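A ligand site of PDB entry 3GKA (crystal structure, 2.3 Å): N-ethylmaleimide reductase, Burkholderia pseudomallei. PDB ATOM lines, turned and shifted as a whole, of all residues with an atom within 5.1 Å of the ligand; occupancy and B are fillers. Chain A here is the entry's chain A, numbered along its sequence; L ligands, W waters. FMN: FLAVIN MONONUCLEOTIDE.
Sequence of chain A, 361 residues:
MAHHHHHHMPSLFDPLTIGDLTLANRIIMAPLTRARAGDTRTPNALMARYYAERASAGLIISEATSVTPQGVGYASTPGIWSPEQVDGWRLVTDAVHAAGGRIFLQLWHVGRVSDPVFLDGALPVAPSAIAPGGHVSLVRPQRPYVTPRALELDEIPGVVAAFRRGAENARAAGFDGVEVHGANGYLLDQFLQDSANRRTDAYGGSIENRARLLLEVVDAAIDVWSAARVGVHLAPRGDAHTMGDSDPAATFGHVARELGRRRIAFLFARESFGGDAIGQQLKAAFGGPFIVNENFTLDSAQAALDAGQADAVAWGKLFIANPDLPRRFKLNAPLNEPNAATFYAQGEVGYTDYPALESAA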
ATOM      1  N   ALA A  30      14.267  19.455 -15.745  1.00  0.00           N
ATOM      2  CA  ALA A  30      13.905  20.642 -14.991  1.00  0.00           C
ATOM      3  C   ALA A  30      12.803  21.416 -15.727  1.00  0.00           C
ATOM      4  O   ALA A  30      12.670  21.312 -16.948  1.00  0.00           O
ATOM      5  CB  ALA A  30      15.127  21.528 -14.801  1.00  0.00           C
ATOM      6  N   PRO A  31      11.991  22.182 -14.977  1.00  0.00           N
ATOM      7  CA  PRO A  31      10.949  22.992 -15.616  1.00  0.00           C
ATOM      8  C   PRO A  31      11.576  24.072 -16.481  1.00  0.00           C
ATOM      9  O   PRO A  31      12.474  24.785 -16.021  1.00  0.00           O
ATOM     10  CB  PRO A  31      10.206  23.600 -14.421  1.00  0.00           C
ATOM     11  CG  PRO A  31      11.218  23.621 -13.339  1.00  0.00           C
ATOM     12  CD  PRO A  31      12.018  22.380 -13.521  1.00  0.00           C
ATOM     13  N   LEU A  32      11.148  24.174 -17.732  1.00  0.00           N
ATOM     14  CA  LEU A  32      11.712  25.156 -18.669  1.00  0.00           C
ATOM     15  C   LEU A  32      10.645  25.880 -19.474  1.00  0.00           C
ATOM     16  O   LEU A  32      10.069  25.307 -20.396  1.00  0.00           O
ATOM     17  CB  LEU A  32      12.686  24.466 -19.622  1.00  0.00           C
ATOM     18  CG  LEU A  32      13.921  23.825 -18.993  1.00  0.00           C
ATOM     19  CD1 LEU A  32      14.392  22.630 -19.820  1.00  0.00           C
ATOM     20  CD2 LEU A  32      15.028  24.859 -18.841  1.00  0.00           C
ATOM     21  N   THR A  33      10.398  27.137 -19.106  1.00  0.00           N
ATOM     22  CA  THR A  33       9.602  28.059 -19.923  1.00  0.00           C
ATOM     23  C   THR A  33      10.233  28.243 -21.297  1.00  0.00           C
ATOM     24  O   THR A  33      11.397  28.648 -21.401  1.00  0.00           O
ATOM     25  CB  THR A  33       9.492  29.457 -19.240  1.00  0.00           C
ATOM     26  OG1 THR A  33       8.728  29.345 -18.029  1.00  0.00           O
ATOM     27  CG2 THR A  33       8.837  30.468 -20.170  1.00  0.00           C
ATOM     28  N   ARG A  34       9.476  27.917 -22.344  1.00  0.00           N
ATOM     29  CA  ARG A  34       9.937  27.992 -23.728  1.00  0.00           C
ATOM     30  C   ARG A  34       9.056  28.858 -24.632  1.00  0.00           C
ATOM     31  O   ARG A  34       9.441  29.177 -25.752  1.00  0.00           O
ATOM     32  CB  ARG A  34      10.033  26.598 -24.342  1.00  0.00           C
ATOM     33  CG  ARG A  34      10.867  25.596 -23.564  1.00  0.00           C
ATOM     34  CD  ARG A  34      12.309  26.047 -23.342  1.00  0.00           C
ATOM     35  NE  ARG A  34      12.975  26.424 -24.588  1.00  0.00           N
ATOM     36  CZ  ARG A  34      13.463  25.564 -25.477  1.00  0.00           C
ATOM     37  NH1 ARG A  34      13.370  24.254 -25.297  1.00  0.00           N
ATOM     38  NH2 ARG A  34      14.044  26.023 -26.578  1.00  0.00           N
ATOM     39  N   GLU A  63       7.277  23.140 -18.024  1.00  0.00           N
ATOM     40  CA  GLU A  63       7.375  24.595 -17.945  1.00  0.00           C
ATOM     41  C   GLU A  63       6.364  25.163 -16.952  1.00  0.00           C
ATOM     42  O   GLU A  63       5.271  24.612 -16.779  1.00  0.00           O
ATOM     43  CB  GLU A  63       7.086  25.189 -19.310  1.00  0.00           C
ATOM     44  CG  GLU A  63       5.666  24.959 -19.789  1.00  0.00           C
ATOM     45  CD  GLU A  63       5.585  24.952 -21.293  1.00  0.00           C
ATOM     46  OE1 GLU A  63       5.236  26.007 -21.872  1.00  0.00           O
ATOM     47  OE2 GLU A  63       5.908  23.900 -21.887  1.00  0.00           O
ATOM     48  N   ALA A  64       6.723  26.271 -16.335  1.00  0.00           N
ATOM     49  CA  ALA A  64       5.839  26.957 -15.407  1.00  0.00           C
ATOM     50  C   ALA A  64       4.521  27.298 -16.110  1.00  0.00           C
ATOM     51  O   ALA A  64       4.533  27.760 -17.243  1.00  0.00           O
ATOM     52  CB  ALA A  64       6.516  28.210 -14.865  1.00  0.00           C
ATOM     53  N   GLN A 106       4.073  22.103 -13.418  1.00  0.00           N
ATOM     54  CA  GLN A 106       4.492  23.155 -12.500  1.00  0.00           C
ATOM     55  C   GLN A 106       3.404  24.239 -12.411  1.00  0.00           C
ATOM     56  O   GLN A 106       3.115  24.904 -13.400  1.00  0.00           O
ATOM     57  CB  GLN A 106       5.827  23.769 -12.904  1.00  0.00           C
ATOM     58  CG  GLN A 106       6.304  24.828 -11.918  1.00  0.00           C
ATOM     59  CD  GLN A 106       7.698  25.328 -12.192  1.00  0.00           C
ATOM     60  OE1 GLN A 106       7.954  25.986 -13.203  1.00  0.00           O
ATOM     61  NE2 GLN A 106       8.608  25.042 -11.269  1.00  0.00           N
ATOM     62  N   HIS A 181       5.304  25.904  -7.607  1.00  0.00           N
ATOM     63  CA  HIS A 181       6.428  26.787  -7.911  1.00  0.00           C
ATOM     64  C   HIS A 181       6.636  27.795  -6.789  1.00  0.00           C
ATOM     65  O   HIS A 181       6.091  28.902  -6.826  1.00  0.00           O
ATOM     66  CB  HIS A 181       6.196  27.519  -9.228  1.00  0.00           C
ATOM     67  CG  HIS A 181       7.434  28.104  -9.820  1.00  0.00           C
ATOM     68  ND1 HIS A 181       8.573  28.344  -9.076  1.00  0.00           N
ATOM     69  CD2 HIS A 181       7.710  28.507 -11.081  1.00  0.00           C
ATOM     70  CE1 HIS A 181       9.501  28.857  -9.861  1.00  0.00           C
ATOM     71  NE2 HIS A 181       9.006  28.962 -11.084  1.00  0.00           N
ATOM     72  N   ASN A 184      12.267  31.218  -7.399  1.00  0.00           N
ATOM     73  CA  ASN A 184      12.651  32.173  -8.441  1.00  0.00           C
ATOM     74  C   ASN A 184      11.960  33.519  -8.362  1.00  0.00           C
ATOM     75  O   ASN A 184      11.772  34.186  -9.365  1.00  0.00           O
ATOM     76  CB  ASN A 184      12.513  31.548  -9.828  1.00  0.00           C
ATOM     77  CG  ASN A 184      13.299  30.248  -9.954  1.00  0.00           C
ATOM     78  OD1 ASN A 184      14.163  29.951  -9.130  1.00  0.00           O
ATOM     79  ND2 ASN A 184      12.992  29.472 -10.983  1.00  0.00           N
ATOM     80  N   HIS A 233       8.977  23.290  -5.450  1.00  0.00           N
ATOM     81  CA  HIS A 233      10.208  23.852  -5.967  1.00  0.00           C
ATOM     82  C   HIS A 233      10.639  25.039  -5.133  1.00  0.00           C
ATOM     83  O   HIS A 233       9.825  25.906  -4.827  1.00  0.00           O
ATOM     84  CB  HIS A 233       9.982  24.314  -7.400  1.00  0.00           C
ATOM     85  CG  HIS A 233      11.206  24.803  -8.083  1.00  0.00           C
ATOM     86  ND1 HIS A 233      12.478  24.472  -7.664  1.00  0.00           N
ATOM     87  CD2 HIS A 233      11.360  25.597  -9.169  1.00  0.00           C
ATOM     88  CE1 HIS A 233      13.369  25.049  -8.457  1.00  0.00           C
ATOM     89  NE2 HIS A 233      12.713  25.734  -9.375  1.00  0.00           N
ATOM     90  N   PHE A 268      12.381  19.926  -4.754  1.00  0.00           N
ATOM     91  CA  PHE A 268      13.296  20.321  -5.840  1.00  0.00           C
ATOM     92  C   PHE A 268      13.923  21.636  -5.438  1.00  0.00           C
ATOM     93  O   PHE A 268      13.224  22.623  -5.278  1.00  0.00           O
ATOM     94  CB  PHE A 268      12.518  20.511  -7.146  1.00  0.00           C
ATOM     95  CG  PHE A 268      13.380  20.726  -8.382  1.00  0.00           C
ATOM     96  CD1 PHE A 268      13.208  19.936  -9.510  1.00  0.00           C
ATOM     97  CD2 PHE A 268      14.330  21.741  -8.439  1.00  0.00           C
ATOM     98  CE1 PHE A 268      13.983  20.133 -10.649  1.00  0.00           C
ATOM     99  CE2 PHE A 268      15.101  21.951  -9.580  1.00  0.00           C
ATOM    100  CZ  PHE A 268      14.930  21.145 -10.682  1.00  0.00           C
ATOM    101  N   ARG A 270      16.620  24.498  -6.609  1.00  0.00           N
ATOM    102  CA  ARG A 270      17.572  25.116  -7.538  1.00  0.00           C
ATOM    103  C   ARG A 270      18.632  25.804  -6.688  1.00  0.00           C
ATOM    104  O   ARG A 270      18.361  26.837  -6.076  1.00  0.00           O
ATOM    105  CB  ARG A 270      16.917  26.127  -8.468  1.00  0.00           C
ATOM    106  CG  ARG A 270      17.944  26.895  -9.310  1.00  0.00           C
ATOM    107  CD  ARG A 270      17.331  27.909 -10.279  1.00  0.00           C
ATOM    108  NE  ARG A 270      16.815  29.102  -9.622  1.00  0.00           N
ATOM    109  CZ  ARG A 270      17.560  30.071  -9.094  1.00  0.00           C
ATOM    110  NH1 ARG A 270      18.892  30.012  -9.102  1.00  0.00           N
ATOM    111  NH2 ARG A 270      16.969  31.122  -8.518  1.00  0.00           N
ATOM    112  N   ASN A 293      19.822  20.657  -8.297  1.00  0.00           N
ATOM    113  CA  ASN A 293      19.835  21.258  -9.630  1.00  0.00           C
ATOM    114  C   ASN A 293      20.671  22.521  -9.676  1.00  0.00           C
ATOM    115  O   ASN A 293      20.772  23.234  -8.677  1.00  0.00           O
ATOM    116  CB  ASN A 293      18.390  21.582 -10.034  1.00  0.00           C
ATOM    117  CG  ASN A 293      18.307  22.488 -11.241  1.00  0.00           C
ATOM    118  OD1 ASN A 293      18.013  23.669 -11.112  1.00  0.00           O
ATOM    119  ND2 ASN A 293      18.608  21.952 -12.416  1.00  0.00           N
ATOM    120  N   GLU A 294      21.265  22.771 -10.858  1.00  0.00           N
ATOM    121  CA  GLU A 294      21.955  24.017 -11.228  1.00  0.00           C
ATOM    122  C   GLU A 294      23.446  23.775 -11.422  1.00  0.00           C
ATOM    123  O   GLU A 294      24.157  23.446 -10.483  1.00  0.00           O
ATOM    124  CB  GLU A 294      21.704  25.162 -10.247  1.00  0.00           C
ATOM    125  CG  GLU A 294      22.140  26.525 -10.766  1.00  0.00           C
ATOM    126  CD  GLU A 294      21.597  27.673  -9.927  1.00  0.00           C
ATOM    127  OE1 GLU A 294      21.026  28.632 -10.502  1.00  0.00           O
ATOM    128  OE2 GLU A 294      21.754  27.637  -8.689  1.00  0.00           O
ATOM    129  N   ASN A 295      23.896  23.920 -12.674  1.00  0.00           N
ATOM    130  CA  ASN A 295      25.307  23.767 -13.054  1.00  0.00           C
ATOM    131  C   ASN A 295      25.895  22.399 -12.747  1.00  0.00           C
ATOM    132  O   ASN A 295      27.090  22.295 -12.432  1.00  0.00           O
ATOM    133  CB  ASN A 295      26.175  24.864 -12.399  1.00  0.00           C
ATOM    134  CG  ASN A 295      25.797  26.268 -12.841  1.00  0.00           C
ATOM    135  OD1 ASN A 295      25.252  26.468 -13.937  1.00  0.00           O
ATOM    136  ND2 ASN A 295      26.112  27.252 -12.010  1.00  0.00           N
ATOM    137  N   PHE A 296      25.082  21.344 -12.843  1.00  0.00           N
ATOM    138  CA  PHE A 296      25.557  19.985 -12.597  1.00  0.00           C
ATOM    139  C   PHE A 296      26.079  19.331 -13.869  1.00  0.00           C
ATOM    140  O   PHE A 296      25.536  19.534 -14.951  1.00  0.00           O
ATOM    141  CB  PHE A 296      24.434  19.101 -12.010  1.00  0.00           C
ATOM    142  CG  PHE A 296      24.322  19.193 -10.526  1.00  0.00           C
ATOM    143  CD1 PHE A 296      24.957  18.278  -9.715  1.00  0.00           C
ATOM    144  CD2 PHE A 296      23.602  20.218  -9.938  1.00  0.00           C
ATOM    145  CE1 PHE A 296      24.859  18.375  -8.332  1.00  0.00           C
ATOM    146  CE2 PHE A 296      23.514  20.309  -8.564  1.00  0.00           C
ATOM    147  CZ  PHE A 296      24.146  19.391  -7.766  1.00  0.00           C
ATOM    148  N   ALA A 314      18.406  17.158 -11.492  1.00  0.00           N
ATOM    149  CA  ALA A 314      17.711  17.747 -12.638  1.00  0.00           C
ATOM    150  C   ALA A 314      18.635  18.634 -13.453  1.00  0.00           C
ATOM    151  O   ALA A 314      19.481  19.350 -12.909  1.00  0.00           O
ATOM    152  CB  ALA A 314      16.502  18.532 -12.176  1.00  0.00           C
ATOM    153  N   TRP A 315      18.445  18.577 -14.771  1.00  0.00           N
ATOM    154  CA  TRP A 315      19.119  19.446 -15.709  1.00  0.00           C
ATOM    155  C   TRP A 315      18.077  20.227 -16.490  1.00  0.00           C
ATOM    156  O   TRP A 315      17.025  19.700 -16.862  1.00  0.00           O
ATOM    157  CB  TRP A 315      19.965  18.626 -16.691  1.00  0.00           C
ATOM    158  CG  TRP A 315      21.249  18.121 -16.123  1.00  0.00           C
ATOM    159  CD1 TRP A 315      22.479  18.700 -16.234  1.00  0.00           C
ATOM    160  CD2 TRP A 315      21.441  16.905 -15.393  1.00  0.00           C
ATOM    161  NE1 TRP A 315      23.425  17.928 -15.608  1.00  0.00           N
ATOM    162  CE2 TRP A 315      22.819  16.818 -15.091  1.00  0.00           C
ATOM    163  CE3 TRP A 315      20.593  15.875 -14.966  1.00  0.00           C
ATOM    164  CZ2 TRP A 315      23.356  15.754 -14.369  1.00  0.00           C
ATOM    165  CZ3 TRP A 315      21.127  14.816 -14.253  1.00  0.00           C
ATOM    166  CH2 TRP A 315      22.494  14.761 -13.963  1.00  0.00           C
ATOM    167  N   GLY A 316      18.372  21.504 -16.732  1.00  0.00           N
ATOM    168  CA  GLY A 316      17.527  22.362 -17.545  1.00  0.00           C
ATOM    169  C   GLY A 316      18.127  22.536 -18.924  1.00  0.00           C
ATOM    170  O   GLY A 316      17.701  21.896 -19.897  1.00  0.00           O
ATOM    171  N   LYS A 317      19.137  23.399 -18.998  1.00  0.00           N
ATOM    172  CA  LYS A 317      19.740  23.782 -20.277  1.00  0.00           C
ATOM    173  C   LYS A 317      20.184  22.580 -21.133  1.00  0.00           C
ATOM    174  O   LYS A 317      19.962  22.568 -22.337  1.00  0.00           O
ATOM    175  CB  LYS A 317      20.885  24.782 -20.049  1.00  0.00           C
ATOM    176  CG  LYS A 317      20.342  26.165 -19.660  1.00  0.00           C
ATOM    177  CD  LYS A 317      21.428  27.229 -19.482  1.00  0.00           C
ATOM    178  CE  LYS A 317      22.250  26.991 -18.210  1.00  0.00           C
ATOM    179  NZ  LYS A 317      21.410  26.943 -16.955  1.00  0.00           N
ATOM    180  N   LEU A 318      20.760  21.558 -20.513  1.00  0.00           N
ATOM    181  CA  LEU A 318      21.197  20.378 -21.254  1.00  0.00           C
ATOM    182  C   LEU A 318      20.038  19.608 -21.868  1.00  0.00           C
ATOM    183  O   LEU A 318      20.178  19.082 -22.959  1.00  0.00           O
ATOM    184  CB  LEU A 318      22.065  19.469 -20.396  1.00  0.00           C
ATOM    185  CG  LEU A 318      23.499  19.964 -20.207  1.00  0.00           C
ATOM    186  CD1 LEU A 318      24.331  18.988 -19.375  1.00  0.00           C
ATOM    187  CD2 LEU A 318      24.189  20.243 -21.559  1.00  0.00           C
ATOM    188  N   ILE A 320      17.210  21.020 -22.854  1.00  0.00           N
ATOM    189  CA  ILE A 320      16.864  21.844 -24.007  1.00  0.00           C
ATOM    190  C   ILE A 320      17.582  21.338 -25.254  1.00  0.00           C
ATOM    191  O   ILE A 320      16.955  21.083 -26.272  1.00  0.00           O
ATOM    192  CB  ILE A 320      17.227  23.336 -23.776  1.00  0.00           C
ATOM    193  CG1 ILE A 320      16.248  23.985 -22.797  1.00  0.00           C
ATOM    194  CG2 ILE A 320      17.262  24.103 -25.091  1.00  0.00           C
ATOM    195  CD1 ILE A 320      16.643  25.377 -22.367  1.00  0.00           C
ATOM    196  N   PHE A 343      15.793  30.025 -26.890  1.00  0.00           N
ATOM    197  CA  PHE A 343      15.173  29.613 -25.622  1.00  0.00           C
ATOM    198  C   PHE A 343      13.717  30.053 -25.532  1.00  0.00           C
ATOM    199  O   PHE A 343      12.871  29.299 -25.074  1.00  0.00           O
ATOM    200  CB  PHE A 343      15.947  30.183 -24.434  1.00  0.00           C
ATOM    201  CG  PHE A 343      17.232  29.434 -24.101  1.00  0.00           C
ATOM    202  CD1 PHE A 343      17.688  28.372 -24.878  1.00  0.00           C
ATOM    203  CD2 PHE A 343      17.991  29.852 -23.012  1.00  0.00           C
ATOM    204  CE1 PHE A 343      18.878  27.725 -24.544  1.00  0.00           C
ATOM    205  CE2 PHE A 343      19.178  29.210 -22.686  1.00  0.00           C
ATOM    206  CZ  PHE A 343      19.624  28.146 -23.460  1.00  0.00           C
ATOM    207  N   TYR A 344      13.442  31.267 -25.982  1.00  0.00           N
ATOM    208  CA  TYR A 344      12.098  31.861 -25.867  1.00  0.00           C
ATOM    209  C   TYR A 344      11.437  32.203 -27.201  1.00  0.00           C
ATOM    210  O   TYR A 344      10.358  32.783 -27.211  1.00  0.00           O
ATOM    211  CB  TYR A 344      12.164  33.114 -24.996  1.00  0.00           C
ATOM    212  CG  TYR A 344      12.871  32.894 -23.668  1.00  0.00           C
ATOM    213  CD1 TYR A 344      12.235  32.222 -22.626  1.00  0.00           C
ATOM    214  CD2 TYR A 344      14.160  33.347 -23.459  1.00  0.00           C
ATOM    215  CE1 TYR A 344      12.870  32.023 -21.393  1.00  0.00           C
ATOM    216  CE2 TYR A 344      14.814  33.143 -22.236  1.00  0.00           C
ATOM    217  CZ  TYR A 344      14.160  32.484 -21.216  1.00  0.00           C
ATOM    218  OH  TYR A 344      14.795  32.285 -20.020  1.00  0.00           O
HETATM  219  N1  FMN L   1      12.565  27.083 -13.574  1.00  0.00           N
HETATM  220  C2  FMN L   1      11.273  26.970 -13.118  1.00  0.00           C
HETATM  221  O2  FMN L   1      11.054  26.622 -11.958  1.00  0.00           O
HETATM  222  N3  FMN L   1      10.211  27.232 -13.959  1.00  0.00           N
HETATM  223  C4  FMN L   1      10.435  27.617 -15.271  1.00  0.00           C
HETATM  224  O4  FMN L   1       9.491  27.761 -16.045  1.00  0.00           O
HETATM  225  C4A FMN L   1      11.746  27.743 -15.727  1.00  0.00           C
HETATM  226  N5  FMN L   1      11.982  28.133 -17.029  1.00  0.00           N
HETATM  227  C5A FMN L   1      13.280  28.253 -17.495  1.00  0.00           C
HETATM  228  C6  FMN L   1      13.516  28.644 -18.797  1.00  0.00           C
HETATM  229  C7  FMN L   1      14.824  28.766 -19.266  1.00  0.00           C
HETATM  230  C7M FMN L   1      15.080  29.168 -20.680  1.00  0.00           C
HETATM  231  C8  FMN L   1      15.892  28.494 -18.409  1.00  0.00           C
HETATM  232  C8M FMN L   1      17.295  28.539 -18.938  1.00  0.00           C
HETATM  233  C9  FMN L   1      15.646  28.109 -17.100  1.00  0.00           C
HETATM  234  C9A FMN L   1      14.348  27.981 -16.638  1.00  0.00           C
HETATM  235  N10 FMN L   1      14.112  27.599 -15.331  1.00  0.00           N
HETATM  236  C10 FMN L   1      12.811  27.476 -14.878  1.00  0.00           C
HETATM  237  C1' FMN L   1      15.254  27.201 -14.457  1.00  0.00           C
HETATM  238  C2' FMN L   1      15.602  25.737 -14.694  1.00  0.00           C
HETATM  239  O2' FMN L   1      14.518  24.928 -14.298  1.00  0.00           O
HETATM  240  C3' FMN L   1      16.844  25.337 -13.922  1.00  0.00           C
HETATM  241  O3' FMN L   1      16.577  25.389 -12.537  1.00  0.00           O
HETATM  242  C4' FMN L   1      18.017  26.260 -14.246  1.00  0.00           C
HETATM  243  O4' FMN L   1      18.122  26.408 -15.643  1.00  0.00           O
HETATM  244  C5' FMN L   1      19.320  25.713 -13.687  1.00  0.00           C
HETATM  245  O5' FMN L   1      19.482  24.374 -14.082  1.00  0.00           O
HETATM  246  P   FMN L   1      20.570  23.981 -15.198  1.00  0.00           P
HETATM  247  O1P FMN L   1      21.906  24.527 -14.778  1.00  0.00           O
HETATM  248  O2P FMN L   1      20.172  24.582 -16.527  1.00  0.00           O
HETATM  249  O3P FMN L   1      20.649  22.481 -15.324  1.00  0.00           O
HETATM  250  O   HOH W   1      24.048  24.783 -16.336  1.00  0.00           O
HETATM  251  O   HOH W   2      22.789  27.446 -14.578  1.00  0.00           O
HETATM  252  O   HOH W   3      21.586  21.108 -13.306  1.00  0.00           O
HETATM  253  O   HOH W   4      21.864  21.875 -17.768  1.00  0.00           O
HETATM  254  O   HOH W   5      19.484  28.707 -16.170  1.00  0.00           O
HETATM  255  O   HOH W   6      11.293  30.210 -13.159  1.00  0.00           O
HETATM  256  O   HOH W   7      14.303  26.357 -11.282  1.00  0.00           O
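Merely in contact with the ligand: Ala 30 (3.5 Å), Leu 32 (3.4 Å), Asn 184 (3.6 Å), Arg 270 (3.5 Å), Glu 294 (3.6 Å), Trp 315 (3.4 Å), Phe 343 (3.8 Å) and Tyr 344 (3.2 Å). Hydrophobic or aromatic side chains that line the ligand: Ala 30, Pro 31, Leu 32, Ala 64, His 181, His 233, Phe 343 and Tyr 344. Within 4 Å of the ligand: Ala 30, Pro 31, Leu 32, Thr 33, Ala 64, Gln 106, His 181, Asn 184, His 233, Arg 270, Asn 293, Glu 294, Asn 295, Trp 315, Gly 316, Lys 317, Phe 343 and Tyr 344. Along chain A the residues within 4 Å of the ligand span positions 30 to 344.
Water W3 lies within hydrogen-bond range of O3P of the ligand (2.6 Å), O of Ala 314 (2.8 Å), N of Glu 294 (3.0 Å) and ND2 of Asn 293 (3.2 Å). Water W1 lies within hydrogen-bond range of O1P of the ligand (2.7 Å), OD1 of Asn 295 (3.2 Å) and NZ of Lys 317 (3.5 Å). Water W5 bridges O4' of the ligand (2.7 Å) and NZ of Lys 317 (2.7 Å). Water W7 lies within hydrogen-bond range of NE2 of His 233 (2.6 Å), O3' of the ligand (2.8 Å) and ND2 of Asn 184 (3.4 Å). Water W4 lies within hydrogen-bond range of an oxygen (O3P) of the ligand (2.8 Å), the backbone NH of Leu 318 (3.0 Å) and the backbone NH of Lys 317 (3.4 Å). Water W6 lies within hydrogen-bond range of ND2 of Asn 184 (2.9 Å), N3 of the ligand (3.3 Å) and NE2 of His 181 (3.3 Å).
The backbone carbonyl oxygen (O) of Phe 343 is in hydrogen-bond range of the guanidinium group (NE) of Arg 34 (2.9 Å). The guanidinium group of Arg 270 is in hydrogen-bond range of the side-chain amide oxygen of Asn 184, 2.8 Å away. The backbone carbonyl oxygen (O) of Phe 296 is in hydrogen-bond range of the indole nitrogen (NE1) of Trp 315 (2.7 Å). O of Trp 315 is in hydrogen-bond range of N of Ala 30, 3.0 Å away. ND2 of Asn 293 is in hydrogen-bond range of O of Ala 314. The backbone NH (N) of Ala 64 sits close to the side-chain amide oxygen (OE1) of Gln 106 (3.4 Å). NH1 of Arg 270 is in salt-bridge range of OE1 of Glu 294 (2.9 Å). A ring nitrogen (ND1) of His 233 lies within hydrogen-bond range of the backbone carbonyl oxygen (O) of Phe 268, at 3.1 Å.
N of Asn 295 is in hydrogen-bond range of O1P of the ligand (3.0 Å). N5 of the ligand sits at hydrogen-bond distance from N of Thr 33 (2.8 Å). N of Lys 317 sits at hydrogen-bond distance from O2P of the ligand, at 2.9 Å. NZ of Lys 317 lies within salt-bridge range of O2P of the ligand (2.7 Å). The backbone NH of Gly 316 is in hydrogen-bond range of an oxygen (O3P) of the ligand, 2.8 Å away. The side-chain amide oxygen (OE1) of Gln 106 is in hydrogen-bond range of a nitrogen (N3) of the ligand, 2.7 Å away. A ring nitrogen (NE2) of His 233 lies close to an oxygen (O2) of the ligand, 3.2 Å away. An oxygen (O2') of the ligand lies within hydrogen-bond range of the backbone carbonyl oxygen of Pro 31 (2.7 Å). N of Ala 64 lies within hydrogen-bond range of O4 of the ligand (3.2 Å). O3' of the ligand lies within hydrogen-bond range of OD1 of Asn 293 (2.7 Å). A ring nitrogen (NE2) of His 181 is in hydrogen-bond range of an oxygen (O2) of the ligand, at 3.2 Å. The side-chain hydroxyl of Thr 33 is in hydrogen-bond range of an oxygen (O4) of the ligand (2.7 Å).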
